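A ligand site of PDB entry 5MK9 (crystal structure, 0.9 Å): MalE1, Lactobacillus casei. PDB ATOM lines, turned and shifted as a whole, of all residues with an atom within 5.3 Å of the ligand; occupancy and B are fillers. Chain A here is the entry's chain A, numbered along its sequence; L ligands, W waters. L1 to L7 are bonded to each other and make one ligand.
O2 of LG5 L5 is in hydrogen-bond range of OD1 of Asn 50 (2.6 Å). O1 of LG2 L2 sits close to O of Asn 46 (3.3 Å). OD1 of Asn 46 lies within hydrogen-bond range of O1 of LIG L1 (2.6 Å). The side-chain carboxylate (OD2) of Asp 16 is in hydrogen-bond range of an oxygen (O1) of LG4 L4, at 2.7 Å. The side-chain carboxylate (OD1) of Asp 71 is in hydrogen-bond range of an oxygen (O1) of LG7 L7 (2.7 Å). OE1 of Gln 119 sits at hydrogen-bond distance from O1 of LG6 L6, 2.7 Å away. O1 of LG5 L5 is in hydrogen-bond range of NZ of Lys 52, at 2.8 Å. O2 of LG7 L7 lies within hydrogen-bond range of NE2 of Gln 72. An oxygen (O1) of LG5 L5 is in hydrogen-bond range of the backbone carbonyl oxygen (O) of Ala 49 (3.1 Å). The side-chain amide nitrogen (ND2) of Asn 153 sits at hydrogen-bond distance from an oxygen (O5) of LG6 L6, at 3.2 Å. An oxygen (O2) of LG2 L2 lies within hydrogen-bond range of the backbone NH (N) of Thr 17. N of Gly 47 lies within hydrogen-bond range of O1 of LG2 L2, 3.5 Å away. OE1 of Glu 262 lies within hydrogen-bond range of O1 of LG6 L6 (3.5 Å).
Water W4 lies within hydrogen-bond range of an oxygen (O2) of LIG L1 and the backbone carbonyl oxygen of Pro 45. Water W16 lies within hydrogen-bond range of O1 of LG4 L4, O of Thr 17 and OE1 of Gln 19. Water W1 lies within hydrogen-bond range of the side-chain hydroxyl of Ser 48 (2.6 Å), the side-chain carboxylate of Glu 262 (2.6 Å) and an oxygen (O1) of LG6 L6 (2.8 Å). Water W14 lies within hydrogen-bond range of O1 of LG2 L2, OG1 of Thr 17, O of Ser 44 and N of Gly 47. Water W3 lies within hydrogen-bond range of the side-chain hydroxyl (OH) of Tyr 155, the side-chain amide oxygen (OE1) of Gln 119 and an oxygen (O2) of LG6 L6. Water W2 lies within hydrogen-bond range of the backbone NH of Ala 154 (2.9 Å) and an oxygen (O5) of LG7 L7 (2.9 Å).
Merely in contact with the ligand: Gln 19 (3.8 Å), Pro 45 (3.996 Å), Ala 69 (3.2 Å), Tyr 155 (3.6 Å), Trp 225 (3.5 Å), Met 334 (3.7 Å) and Trp 344 (3.7 Å). Hydrophobic or aromatic side chains that line the ligand: Ala 49, Ala 69, Tyr 155, Trp 225, Met 334 and Trp 344. The nearest printed residue that does not touch the ligand is Ser 48 (4.1 Å).
N of Asp 16 lies close to NE2 of Gln 19 (3.3 Å). The side-chain carboxylate (OE1) of Glu 67 is in hydrogen-bond range of the backbone NH (N) of Asp 16, at 3.4 Å. The indole nitrogen (NE1) of Trp 344 sits at hydrogen-bond distance from the side-chain carboxylate (OD2) of Asp 71 (2.9 Å). NE2 of Gln 119 is in hydrogen-bond range of OE1 of Glu 262. N of Lys 52 lies within hydrogen-bond range of OE1 of Gln 72, 2.8 Å away. The side-chain amide oxygen (OD1) of Asn 153 is in hydrogen-bond range of the backbone NH (N) of Tyr 155 (2.9 Å). OE2 of Glu 262 sits at hydrogen-bond distance from N of Ala 69, at 3.4 Å. The backbone NH (N) of Gly 47 lies within hydrogen-bond range of the side-chain hydroxyl (OG) of Ser 44 (2.9 Å).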
ATOM      1  N   ASP A  16     -22.798  22.926   6.653  1.00  0.00           N
ATOM      2  CA  ASP A  16     -23.415  21.659   7.007  1.00  0.00           C
ATOM      3  C   ASP A  16     -23.919  20.901   5.776  1.00  0.00           C
ATOM      4  O   ASP A  16     -24.177  21.464   4.718  1.00  0.00           O
ATOM      5  CB  ASP A  16     -24.584  21.896   7.975  1.00  0.00           C
ATOM      6  CG  ASP A  16     -24.125  22.202   9.400  1.00  0.00           C
ATOM      7  OD1 ASP A  16     -22.985  22.671   9.603  1.00  0.00           O
ATOM      8  OD2 ASP A  16     -24.885  21.950  10.354  1.00  0.00           O
ATOM      9  N   THR A  17     -24.067  19.597   5.949  1.00  0.00           N
ATOM     10  CA  THR A  17     -24.609  18.764   4.904  1.00  0.00           C
ATOM     11  C   THR A  17     -25.969  19.305   4.459  1.00  0.00           C
ATOM     12  O   THR A  17     -26.799  19.697   5.279  1.00  0.00           O
ATOM     13  CB  THR A  17     -24.670  17.328   5.409  1.00  0.00           C
ATOM     14  OG1 THR A  17     -23.352  16.987   5.874  1.00  0.00           O
ATOM     15  CG2 THR A  17     -25.101  16.380   4.323  1.00  0.00           C
ATOM     16  N   GLN A  19     -26.278  22.031   2.730  1.00  0.00           N
ATOM     17  CA  GLN A  19     -26.208  23.476   2.538  1.00  0.00           C
ATOM     18  C   GLN A  19     -25.275  23.896   1.410  1.00  0.00           C
ATOM     19  O   GLN A  19     -25.336  25.057   0.989  1.00  0.00           O
ATOM     20  CB  GLN A  19     -25.757  24.165   3.850  1.00  0.00           C
ATOM     21  CG  GLN A  19     -26.666  23.811   5.013  1.00  0.00           C
ATOM     22  CD  GLN A  19     -26.355  24.511   6.298  1.00  0.00           C
ATOM     23  OE1 GLN A  19     -27.107  24.379   7.288  1.00  0.00           O
ATOM     24  NE2 GLN A  19     -25.235  25.184   6.340  1.00  0.00           N
ATOM     25  N   SER A  44     -18.511  20.279   6.164  1.00  0.00           N
ATOM     26  CA  SER A  44     -17.583  19.949   7.220  1.00  0.00           C
ATOM     27  C   SER A  44     -17.673  18.463   7.545  1.00  0.00           C
ATOM     28  O   SER A  44     -18.660  17.792   7.218  1.00  0.00           O
ATOM     29  CB  SER A  44     -17.942  20.713   8.488  1.00  0.00           C
ATOM     30  OG  SER A  44     -19.275  20.389   8.858  1.00  0.00           O
ATOM     31  N   PRO A  45     -16.654  17.928   8.227  1.00  0.00           N
ATOM     32  CA  PRO A  45     -16.697  16.501   8.564  1.00  0.00           C
ATOM     33  C   PRO A  45     -17.933  16.107   9.355  1.00  0.00           C
ATOM     34  O   PRO A  45     -18.520  15.046   9.070  1.00  0.00           O
ATOM     35  CB  PRO A  45     -15.382  16.288   9.320  1.00  0.00           C
ATOM     36  CG  PRO A  45     -14.456  17.287   8.677  1.00  0.00           C
ATOM     37  CD  PRO A  45     -15.312  18.502   8.452  1.00  0.00           C
ATOM     38  N   ASN A  46     -18.337  16.900  10.343  1.00  0.00           N
ATOM     39  CA  ASN A  46     -19.395  16.474  11.254  1.00  0.00           C
ATOM     40  C   ASN A  46     -20.413  17.557  11.583  1.00  0.00           C
ATOM     41  O   ASN A  46     -21.245  17.365  12.477  1.00  0.00           O
ATOM     42  CB  ASN A  46     -18.836  15.886  12.548  1.00  0.00           C
ATOM     43  CG  ASN A  46     -18.065  14.619  12.306  1.00  0.00           C
ATOM     44  OD1 ASN A  46     -18.658  13.558  12.103  1.00  0.00           O
ATOM     45  ND2 ASN A  46     -16.749  14.722  12.285  1.00  0.00           N
ATOM     46  N   GLY A  47     -20.383  18.687  10.887  1.00  0.00           N
ATOM     47  CA  GLY A  47     -21.401  19.704  11.032  1.00  0.00           C
ATOM     48  C   GLY A  47     -21.067  20.763  12.074  1.00  0.00           C
ATOM     49  O   GLY A  47     -20.181  20.604  12.923  1.00  0.00           O
ATOM     50  N   SER A  48     -21.844  21.836  12.015  1.00  0.00           N
ATOM     51  CA  SER A  48     -21.729  22.967  12.915  1.00  0.00           C
ATOM     52  C   SER A  48     -21.896  22.599  14.377  1.00  0.00           C
ATOM     53  O   SER A  48     -21.332  23.275  15.245  1.00  0.00           O
ATOM     54  CB  SER A  48     -22.756  24.022  12.501  1.00  0.00           C
ATOM     55  OG  SER A  48     -24.067  23.497  12.511  1.00  0.00           O
ATOM     56  N   ALA A  49     -22.649  21.532  14.677  1.00  0.00           N
ATOM     57  CA  ALA A  49     -22.822  21.066  16.058  1.00  0.00           C
ATOM     58  C   ALA A  49     -21.568  20.356  16.584  1.00  0.00           C
ATOM     59  O   ALA A  49     -21.520  19.992  17.763  1.00  0.00           O
ATOM     60  CB  ALA A  49     -24.034  20.147  16.143  1.00  0.00           C
ATOM     61  N   ASN A  50     -20.571  20.181  15.733  1.00  0.00           N
ATOM     62  CA  ASN A  50     -19.325  19.488  16.060  1.00  0.00           C
ATOM     63  C   ASN A  50     -18.107  20.302  15.638  1.00  0.00           C
ATOM     64  O   ASN A  50     -17.007  19.744  15.518  1.00  0.00           O
ATOM     65  CB  ASN A  50     -19.283  18.137  15.372  1.00  0.00           C
ATOM     66  CG  ASN A  50     -20.251  17.173  15.971  1.00  0.00           C
ATOM     67  OD1 ASN A  50     -19.968  16.617  17.017  1.00  0.00           O
ATOM     68  ND2 ASN A  50     -21.379  16.976  15.324  1.00  0.00           N
ATOM     69  N   LYS A  52     -16.132  22.553  17.061  1.00  0.00           N
ATOM     70  CA  LYS A  52     -14.944  22.685  17.867  1.00  0.00           C
ATOM     71  C   LYS A  52     -14.090  21.437  17.797  1.00  0.00           C
ATOM     72  O   LYS A  52     -12.867  21.532  17.880  1.00  0.00           O
ATOM     73  CB  LYS A  52     -15.294  23.052  19.291  1.00  0.00           C
ATOM     74  CG  LYS A  52     -16.025  22.002  19.965  1.00  0.00           C
ATOM     75  CD  LYS A  52     -16.418  22.409  21.358  1.00  0.00           C
ATOM     76  CE  LYS A  52     -16.953  21.236  22.149  1.00  0.00           C
ATOM     77  NZ  LYS A  52     -18.202  20.675  21.648  1.00  0.00           N
ATOM     78  N   THR A  53     -14.718  20.266  17.640  1.00  0.00           N
ATOM     79  CA  THR A  53     -13.999  19.007  17.460  1.00  0.00           C
ATOM     80  C   THR A  53     -13.359  18.922  16.077  1.00  0.00           C
ATOM     81  O   THR A  53     -12.180  18.583  15.936  1.00  0.00           O
ATOM     82  CB  THR A  53     -14.952  17.834  17.645  1.00  0.00           C
ATOM     83  OG1 THR A  53     -15.553  17.913  18.939  1.00  0.00           O
ATOM     84  CG2 THR A  53     -14.253  16.501  17.449  1.00  0.00           C
ATOM     85  N   GLU A  67     -18.894  26.895   9.744  1.00  0.00           N
ATOM     86  CA  GLU A  67     -20.156  27.060  10.441  1.00  0.00           C
ATOM     87  C   GLU A  67     -20.022  26.486  11.859  1.00  0.00           C
ATOM     88  O   GLU A  67     -19.450  25.405  12.058  1.00  0.00           O
ATOM     89  CB  GLU A  67     -21.267  26.349   9.657  1.00  0.00           C
ATOM     90  CG  GLU A  67     -22.672  26.805  10.036  1.00  0.00           C
ATOM     91  CD  GLU A  67     -23.764  26.231   9.192  1.00  0.00           C
ATOM     92  OE1 GLU A  67     -23.454  26.008   7.999  1.00  0.00           O
ATOM     93  OE2 GLU A  67     -24.897  26.030   9.655  1.00  0.00           O
ATOM     94  N   ALA A  69     -22.160  26.458  15.882  1.00  0.00           N
ATOM     95  CA  ALA A  69     -23.209  26.851  16.805  1.00  0.00           C
ATOM     96  C   ALA A  69     -22.643  27.704  17.940  1.00  0.00           C
ATOM     97  O   ALA A  69     -21.528  27.477  18.427  1.00  0.00           O
ATOM     98  CB  ALA A  69     -23.880  25.605  17.370  1.00  0.00           C
ATOM     99  N   ASP A  71     -22.939  27.980  21.131  1.00  0.00           N
ATOM    100  CA  ASP A  71     -22.514  27.452  22.421  1.00  0.00           C
ATOM    101  C   ASP A  71     -21.037  27.089  22.461  1.00  0.00           C
ATOM    102  O   ASP A  71     -20.456  27.022  23.555  1.00  0.00           O
ATOM    103  CB  ASP A  71     -23.315  26.203  22.827  1.00  0.00           C
ATOM    104  CG  ASP A  71     -23.154  25.056  21.849  1.00  0.00           C
ATOM    105  OD1 ASP A  71     -23.477  25.253  20.660  1.00  0.00           O
ATOM    106  OD2 ASP A  71     -22.717  23.939  22.277  1.00  0.00           O
ATOM    107  N   GLN A  72     -20.424  26.838  21.299  1.00  0.00           N
ATOM    108  CA  GLN A  72     -19.040  26.371  21.225  1.00  0.00           C
ATOM    109  C   GLN A  72     -18.038  27.529  21.286  1.00  0.00           C
ATOM    110  O   GLN A  72     -16.833  27.284  21.362  1.00  0.00           O
ATOM    111  CB  GLN A  72     -18.854  25.566  19.934  1.00  0.00           C
ATOM    112  CG  GLN A  72     -19.797  24.395  19.899  1.00  0.00           C
ATOM    113  CD  GLN A  72     -19.436  23.359  18.911  1.00  0.00           C
ATOM    114  OE1 GLN A  72     -18.520  23.539  18.108  1.00  0.00           O
ATOM    115  NE2 GLN A  72     -20.133  22.227  18.963  1.00  0.00           N
ATOM    116  N   GLN A 119     -32.196  29.857  15.763  1.00  0.00           N
ATOM    117  CA  GLN A 119     -32.727  28.501  15.830  1.00  0.00           C
ATOM    118  C   GLN A 119     -33.426  28.282  17.161  1.00  0.00           C
ATOM    119  O   GLN A 119     -32.793  28.292  18.208  1.00  0.00           O
ATOM    120  CB  GLN A 119     -31.598  27.484  15.693  1.00  0.00           C
ATOM    121  CG  GLN A 119     -30.920  27.558  14.332  1.00  0.00           C
ATOM    122  CD  GLN A 119     -29.769  26.620  14.189  1.00  0.00           C
ATOM    123  OE1 GLN A 119     -29.210  26.125  15.182  1.00  0.00           O
ATOM    124  NE2 GLN A 119     -29.349  26.385  12.948  1.00  0.00           N
ATOM    125  N   GLN A 121     -36.468  25.395  18.466  1.00  0.00           N
ATOM    126  CA  GLN A 121     -37.332  24.321  18.032  1.00  0.00           C
ATOM    127  C   GLN A 121     -38.798  24.667  18.244  1.00  0.00           C
ATOM    128  O   GLN A 121     -39.173  25.490  19.082  1.00  0.00           O
ATOM    129  CB  GLN A 121     -36.984  22.996  18.711  1.00  0.00           C
ATOM    130  CG  GLN A 121     -35.616  22.485  18.259  1.00  0.00           C
ATOM    131  CD  GLN A 121     -35.288  21.041  18.524  1.00  0.00           C
ATOM    132  OE1 GLN A 121     -34.363  20.519  17.909  1.00  0.00           O
ATOM    133  NE2 GLN A 121     -36.011  20.387  19.428  1.00  0.00           N
ATOM    134  N   ASN A 153     -31.080  13.192  23.594  1.00  0.00           N
ATOM    135  CA  ASN A 153     -30.561  14.449  23.076  1.00  0.00           C
ATOM    136  C   ASN A 153     -30.883  15.550  24.081  1.00  0.00           C
ATOM    137  O   ASN A 153     -32.037  15.958  24.234  1.00  0.00           O
ATOM    138  CB  ASN A 153     -31.171  14.709  21.702  1.00  0.00           C
ATOM    139  CG  ASN A 153     -30.560  15.934  21.055  1.00  0.00           C
ATOM    140  OD1 ASN A 153     -30.204  16.861  21.727  1.00  0.00           O
ATOM    141  ND2 ASN A 153     -30.445  15.942  19.761  1.00  0.00           N
ATOM    142  N   ALA A 154     -29.850  16.017  24.780  1.00  0.00           N
ATOM    143  CA  ALA A 154     -30.041  17.031  25.814  1.00  0.00           C
ATOM    144  C   ALA A 154     -30.476  18.379  25.237  1.00  0.00           C
ATOM    145  O   ALA A 154     -31.064  19.197  25.961  1.00  0.00           O
ATOM    146  CB  ALA A 154     -28.768  17.201  26.633  1.00  0.00           C
ATOM    147  N   TYR A 155     -30.154  18.653  23.972  1.00  0.00           N
ATOM    148  CA  TYR A 155     -30.648  19.858  23.341  1.00  0.00           C
ATOM    149  C   TYR A 155     -32.171  19.865  23.262  1.00  0.00           C
ATOM    150  O   TYR A 155     -32.808  20.922  23.355  1.00  0.00           O
ATOM    151  CB  TYR A 155     -29.999  20.001  21.964  1.00  0.00           C
ATOM    152  CG  TYR A 155     -30.430  21.202  21.164  1.00  0.00           C
ATOM    153  CD1 TYR A 155     -29.764  22.407  21.256  1.00  0.00           C
ATOM    154  CD2 TYR A 155     -31.453  21.090  20.227  1.00  0.00           C
ATOM    155  CE1 TYR A 155     -30.101  23.498  20.447  1.00  0.00           C
ATOM    156  CE2 TYR A 155     -31.789  22.155  19.404  1.00  0.00           C
ATOM    157  CZ  TYR A 155     -31.099  23.349  19.505  1.00  0.00           C
ATOM    158  OH  TYR A 155     -31.452  24.370  18.656  1.00  0.00           O
ATOM    159  N   TRP A 225     -33.722  23.955  10.576  1.00  0.00           N
ATOM    160  CA  TRP A 225     -32.841  23.310   9.627  1.00  0.00           C
ATOM    161  C   TRP A 225     -33.522  22.148   8.888  1.00  0.00           C
ATOM    162  O   TRP A 225     -33.132  21.851   7.762  1.00  0.00           O
ATOM    163  CB  TRP A 225     -31.539  22.860  10.332  1.00  0.00           C
ATOM    164  CG  TRP A 225     -31.832  21.957  11.496  1.00  0.00           C
ATOM    165  CD1 TRP A 225     -32.046  20.605  11.463  1.00  0.00           C
ATOM    166  CD2 TRP A 225     -31.974  22.340  12.868  1.00  0.00           C
ATOM    167  NE1 TRP A 225     -32.317  20.130  12.726  1.00  0.00           N
ATOM    168  CE2 TRP A 225     -32.295  21.178  13.603  1.00  0.00           C
ATOM    169  CE3 TRP A 225     -31.834  23.548  13.555  1.00  0.00           C
ATOM    170  CZ2 TRP A 225     -32.501  21.204  14.980  1.00  0.00           C
ATOM    171  CZ3 TRP A 225     -32.008  23.567  14.926  1.00  0.00           C
ATOM    172  CH2 TRP A 225     -32.347  22.406  15.625  1.00  0.00           C
ATOM    173  N   GLU A 262     -26.799  30.382  14.888  1.00  0.00           N
ATOM    174  CA  GLU A 262     -25.896  29.748  13.940  1.00  0.00           C
ATOM    175  C   GLU A 262     -24.984  30.820  13.375  1.00  0.00           C
ATOM    176  O   GLU A 262     -25.439  31.928  13.069  1.00  0.00           O
ATOM    177  CB  GLU A 262     -26.699  29.052  12.835  1.00  0.00           C
ATOM    178  CG  GLU A 262     -25.892  28.043  12.043  1.00  0.00           C
ATOM    179  CD  GLU A 262     -25.426  26.928  12.897  1.00  0.00           C
ATOM    180  OE1 GLU A 262     -26.231  26.040  13.199  1.00  0.00           O
ATOM    181  OE2 GLU A 262     -24.250  26.975  13.309  1.00  0.00           O
ATOM    182  N   GLN A 300     -34.460  28.514   7.137  1.00  0.00           N
ATOM    183  CA  GLN A 300     -33.877  29.019   8.359  1.00  0.00           C
ATOM    184  C   GLN A 300     -34.117  30.521   8.491  1.00  0.00           C
ATOM    185  O   GLN A 300     -34.288  31.251   7.508  1.00  0.00           O
ATOM    186  CB  GLN A 300     -32.392  28.655   8.463  1.00  0.00           C
ATOM    187  CG  GLN A 300     -32.166  27.160   8.723  1.00  0.00           C
ATOM    188  CD  GLN A 300     -30.981  26.888   9.624  1.00  0.00           C
ATOM    189  OE1 GLN A 300     -30.935  27.381  10.755  1.00  0.00           O
ATOM    190  NE2 GLN A 300     -30.022  26.120   9.126  1.00  0.00           N
ATOM    191  N   MET A 334     -28.479  29.552  24.323  1.00  0.00           N
ATOM    192  CA  MET A 334     -27.486  28.567  24.758  1.00  0.00           C
ATOM    193  C   MET A 334     -26.281  29.297  25.335  1.00  0.00           C
ATOM    194  O   MET A 334     -25.675  30.128  24.626  1.00  0.00           O
ATOM    195  CB  MET A 334     -26.961  27.700  23.624  1.00  0.00           C
ATOM    196  CG  MET A 334     -27.967  26.717  23.065  1.00  0.00           C
ATOM    197  SD  MET A 334     -27.217  25.419  22.041  1.00  0.00           S
ATOM    198  CE  MET A 334     -26.753  26.348  20.585  1.00  0.00           C
ATOM    199  N   TRP A 344     -22.877  19.171  27.978  1.00  0.00           N
ATOM    200  CA  TRP A 344     -23.636  18.335  27.071  1.00  0.00           C
ATOM    201  C   TRP A 344     -23.404  16.853  27.351  1.00  0.00           C
ATOM    202  O   TRP A 344     -24.332  16.045  27.315  1.00  0.00           O
ATOM    203  CB  TRP A 344     -23.296  18.637  25.616  1.00  0.00           C
ATOM    204  CG  TRP A 344     -23.701  19.977  25.125  1.00  0.00           C
ATOM    205  CD1 TRP A 344     -22.863  20.959  24.652  1.00  0.00           C
ATOM    206  CD2 TRP A 344     -25.022  20.508  25.022  1.00  0.00           C
ATOM    207  NE1 TRP A 344     -23.577  22.061  24.268  1.00  0.00           N
ATOM    208  CE2 TRP A 344     -24.912  21.815  24.473  1.00  0.00           C
ATOM    209  CE3 TRP A 344     -26.306  20.024  25.314  1.00  0.00           C
ATOM    210  CZ2 TRP A 344     -26.027  22.605  24.217  1.00  0.00           C
ATOM    211  CZ3 TRP A 344     -27.402  20.804  25.058  1.00  0.00           C
ATOM    212  CH2 TRP A 344     -27.245  22.093  24.541  1.00  0.00           C
ATOM    213  N   ASN A 345     -22.159  16.492  27.661  1.00  0.00           N
ATOM    214  CA  ASN A 345     -21.835  15.093  27.864  1.00  0.00           C
ATOM    215  C   ASN A 345     -22.490  14.544  29.121  1.00  0.00           C
ATOM    216  O   ASN A 345     -22.784  13.341  29.195  1.00  0.00           O
ATOM    217  CB  ASN A 345     -20.318  14.911  27.926  1.00  0.00           C
ATOM    218  CG  ASN A 345     -19.891  13.482  27.687  1.00  0.00           C
ATOM    219  OD1 ASN A 345     -20.173  12.903  26.642  1.00  0.00           O
ATOM    220  ND2 ASN A 345     -19.184  12.913  28.656  1.00  0.00           N
HETATM  221  C1  LIG L   1     -23.043  12.569  14.152  1.00  0.00           C
HETATM  222  C2  LIG L   1     -22.142  12.871  12.990  1.00  0.00           C
HETATM  223  C3  LIG L   1     -22.613  14.155  12.305  1.00  0.00           C
HETATM  224  C4  LIG L   1     -24.088  14.053  12.015  1.00  0.00           C
HETATM  225  C5  LIG L   1     -24.840  13.731  13.279  1.00  0.00           C
HETATM  226  C6  LIG L   1     -26.343  13.528  12.987  1.00  0.00           C
HETATM  227  O1  LIG L   1     -20.806  12.981  13.446  1.00  0.00           O
HETATM  228  O2  LIG L   1     -21.874  14.330  11.121  1.00  0.00           O
HETATM  229  O3  LIG L   1     -24.514  15.332  11.510  1.00  0.00           O
HETATM  230  O4  LIG L   1     -24.379  12.529  13.848  1.00  0.00           O
HETATM  231  O5  LIG L   1     -26.543  12.412  12.109  1.00  0.00           O
HETATM  232  C1  LG2 L   2     -24.841  15.352  10.099  1.00  0.00           C
HETATM  233  C2  LG2 L   2     -24.213  16.562   9.431  1.00  0.00           C
HETATM  234  C3  LG2 L   2     -24.819  17.845   9.972  1.00  0.00           C
HETATM  235  C4  LG2 L   2     -26.325  17.820   9.939  1.00  0.00           C
HETATM  236  C5  LG2 L   2     -26.892  16.530  10.503  1.00  0.00           C
HETATM  237  C6  LG2 L   2     -28.361  16.258  10.190  1.00  0.00           C
HETATM  238  O1  LG2 L   2     -22.792  16.529   9.664  1.00  0.00           O
HETATM  239  O2  LG2 L   2     -24.330  18.932   9.201  1.00  0.00           O
HETATM  240  O3  LG2 L   2     -26.681  19.001  10.716  1.00  0.00           O
HETATM  241  O4  LG2 L   2     -26.220  15.399   9.923  1.00  0.00           O
HETATM  242  O5  LG2 L   2     -28.685  14.899  10.373  1.00  0.00           O
HETATM  243  C1  LG3 L   3     -21.867  13.792  19.318  1.00  0.00           C
HETATM  244  C2  LG3 L   3     -20.785  13.212  18.414  1.00  0.00           C
HETATM  245  C3  LG3 L   3     -21.088  13.535  16.971  1.00  0.00           C
HETATM  246  C4  LG3 L   3     -22.491  13.128  16.627  1.00  0.00           C
HETATM  247  C5  LG3 L   3     -23.502  13.653  17.605  1.00  0.00           C
HETATM  248  C6  LG3 L   3     -24.917  13.121  17.295  1.00  0.00           C
HETATM  249  O1  LG3 L   3     -19.522  13.710  18.779  1.00  0.00           O
HETATM  250  O2  LG3 L   3     -20.141  12.893  16.134  1.00  0.00           O
HETATM  251  O3  LG3 L   3     -22.789  13.500  15.252  1.00  0.00           O
HETATM  252  O4  LG3 L   3     -23.141  13.295  18.936  1.00  0.00           O
HETATM  253  O5  LG3 L   3     -24.937  11.722  17.453  1.00  0.00           O
HETATM  254  C1  LG4 L   4     -28.068  19.375  10.730  1.00  0.00           C
HETATM  255  C2  LG4 L   4     -28.169  20.879  10.846  1.00  0.00           C
HETATM  256  C3  LG4 L   4     -27.764  21.388  12.219  1.00  0.00           C
HETATM  257  C4  LG4 L   4     -28.496  20.581  13.290  1.00  0.00           C
HETATM  258  C5  LG4 L   4     -28.259  19.099  13.081  1.00  0.00           C
HETATM  259  C6  LG4 L   4     -29.021  18.223  14.085  1.00  0.00           C
HETATM  260  O1  LG4 L   4     -27.470  21.558   9.798  1.00  0.00           O
HETATM  261  O2  LG4 L   4     -28.096  22.762  12.291  1.00  0.00           O
HETATM  262  O3  LG4 L   4     -28.009  21.013  14.570  1.00  0.00           O
HETATM  263  O4  LG4 L   4     -28.742  18.752  11.780  1.00  0.00           O
HETATM  264  O5  LG4 L   4     -28.617  16.876  13.897  1.00  0.00           O
HETATM  265  C1  LG5 L   5     -22.459  18.421  21.690  1.00  0.00           C
HETATM  266  C2  LG5 L   5     -21.101  18.239  21.089  1.00  0.00           C
HETATM  267  C3  LG5 L   5     -21.095  17.272  19.930  1.00  0.00           C
HETATM  268  C4  LG5 L   5     -21.775  15.974  20.349  1.00  0.00           C
HETATM  269  C5  LG5 L   5     -23.139  16.259  20.981  1.00  0.00           C
HETATM  270  C6  LG5 L   5     -23.859  15.035  21.527  1.00  0.00           C
HETATM  271  O1  LG5 L   5     -20.553  19.498  20.692  1.00  0.00           O
HETATM  272  O2  LG5 L   5     -19.731  17.052  19.527  1.00  0.00           O
HETATM  273  O3  LG5 L   5     -21.847  15.201  19.150  1.00  0.00           O
HETATM  274  O4  LG5 L   5     -22.989  17.175  22.078  1.00  0.00           O
HETATM  275  O5  LG5 L   5     -23.096  14.402  22.599  1.00  0.00           O
HETATM  276  C1  LG6 L   6     -28.979  21.526  15.446  1.00  0.00           C
HETATM  277  C2  LG6 L   6     -28.471  22.841  16.046  1.00  0.00           C
HETATM  278  C3  LG6 L   6     -27.348  22.600  17.038  1.00  0.00           C
HETATM  279  C4  LG6 L   6     -27.694  21.522  18.028  1.00  0.00           C
HETATM  280  C5  LG6 L   6     -28.198  20.270  17.361  1.00  0.00           C
HETATM  281  C6  LG6 L   6     -28.759  19.267  18.377  1.00  0.00           C
HETATM  282  O1  LG6 L   6     -28.061  23.672  14.988  1.00  0.00           O
HETATM  283  O2  LG6 L   6     -27.064  23.828  17.695  1.00  0.00           O
HETATM  284  O3  LG6 L   6     -26.471  21.195  18.781  1.00  0.00           O
HETATM  285  O4  LG6 L   6     -29.287  20.580  16.491  1.00  0.00           O
HETATM  286  O5  LG6 L   6     -29.097  18.015  17.793  1.00  0.00           O
HETATM  287  C1  LG7 L   7     -26.422  21.659  20.091  1.00  0.00           C
HETATM  288  C2  LG7 L   7     -25.046  22.289  20.335  1.00  0.00           C
HETATM  289  C3  LG7 L   7     -23.948  21.260  20.226  1.00  0.00           C
HETATM  290  C4  LG7 L   7     -24.222  20.058  21.093  1.00  0.00           C
HETATM  291  C5  LG7 L   7     -25.630  19.542  20.871  1.00  0.00           C
HETATM  292  C6  LG7 L   7     -26.011  18.489  21.937  1.00  0.00           C
HETATM  293  O1  LG7 L   7     -24.885  23.352  19.408  1.00  0.00           O
HETATM  294  O2  LG7 L   7     -22.644  21.814  20.527  1.00  0.00           O
HETATM  295  O3  LG7 L   7     -23.271  19.039  20.689  1.00  0.00           O
HETATM  296  O4  LG7 L   7     -26.602  20.579  21.004  1.00  0.00           O
HETATM  297  O5  LG7 L   7     -27.166  17.777  21.595  1.00  0.00           O
HETATM  298  O   HOH W   1     -25.309  24.109  14.724  1.00  0.00           O
HETATM  299  O   HOH W   2     -27.262  15.680  23.603  1.00  0.00           O
HETATM  300  O   HOH W   3     -29.189  25.704  17.946  1.00  0.00           O
HETATM  301  O   HOH W   4     -20.874  13.700   8.922  1.00  0.00           O
HETATM  302  O   HOH W   5     -24.135  17.461  13.519  1.00  0.00           O
HETATM  303  O   HOH W   6     -26.514  15.879  19.710  1.00  0.00           O
HETATM  304  O   HOH W   7     -27.613  24.914  10.411  1.00  0.00           O
HETATM  305  O   HOH W   8     -26.017  16.460  14.893  1.00  0.00           O
HETATM  306  O   HOH W   9     -21.774  15.480  24.297  1.00  0.00           O
HETATM  307  O   HOH W  10     -24.853  14.922  24.830  1.00  0.00           O
HETATM  308  O   HOH W  11     -19.912  10.144  16.185  1.00  0.00           O
HETATM  309  O   HOH W  12     -31.478  17.417  16.473  1.00  0.00           O
HETATM  310  O   HOH W  13     -27.329  16.039  17.285  1.00  0.00           O
HETATM  311  O   HOH W  14     -21.567  18.257   7.767  1.00  0.00           O
HETATM  312  O   HOH W  15     -27.130  12.607   9.362  1.00  0.00           O
HETATM  313  O   HOH W  16     -28.503  21.390   7.301  1.00  0.00           O
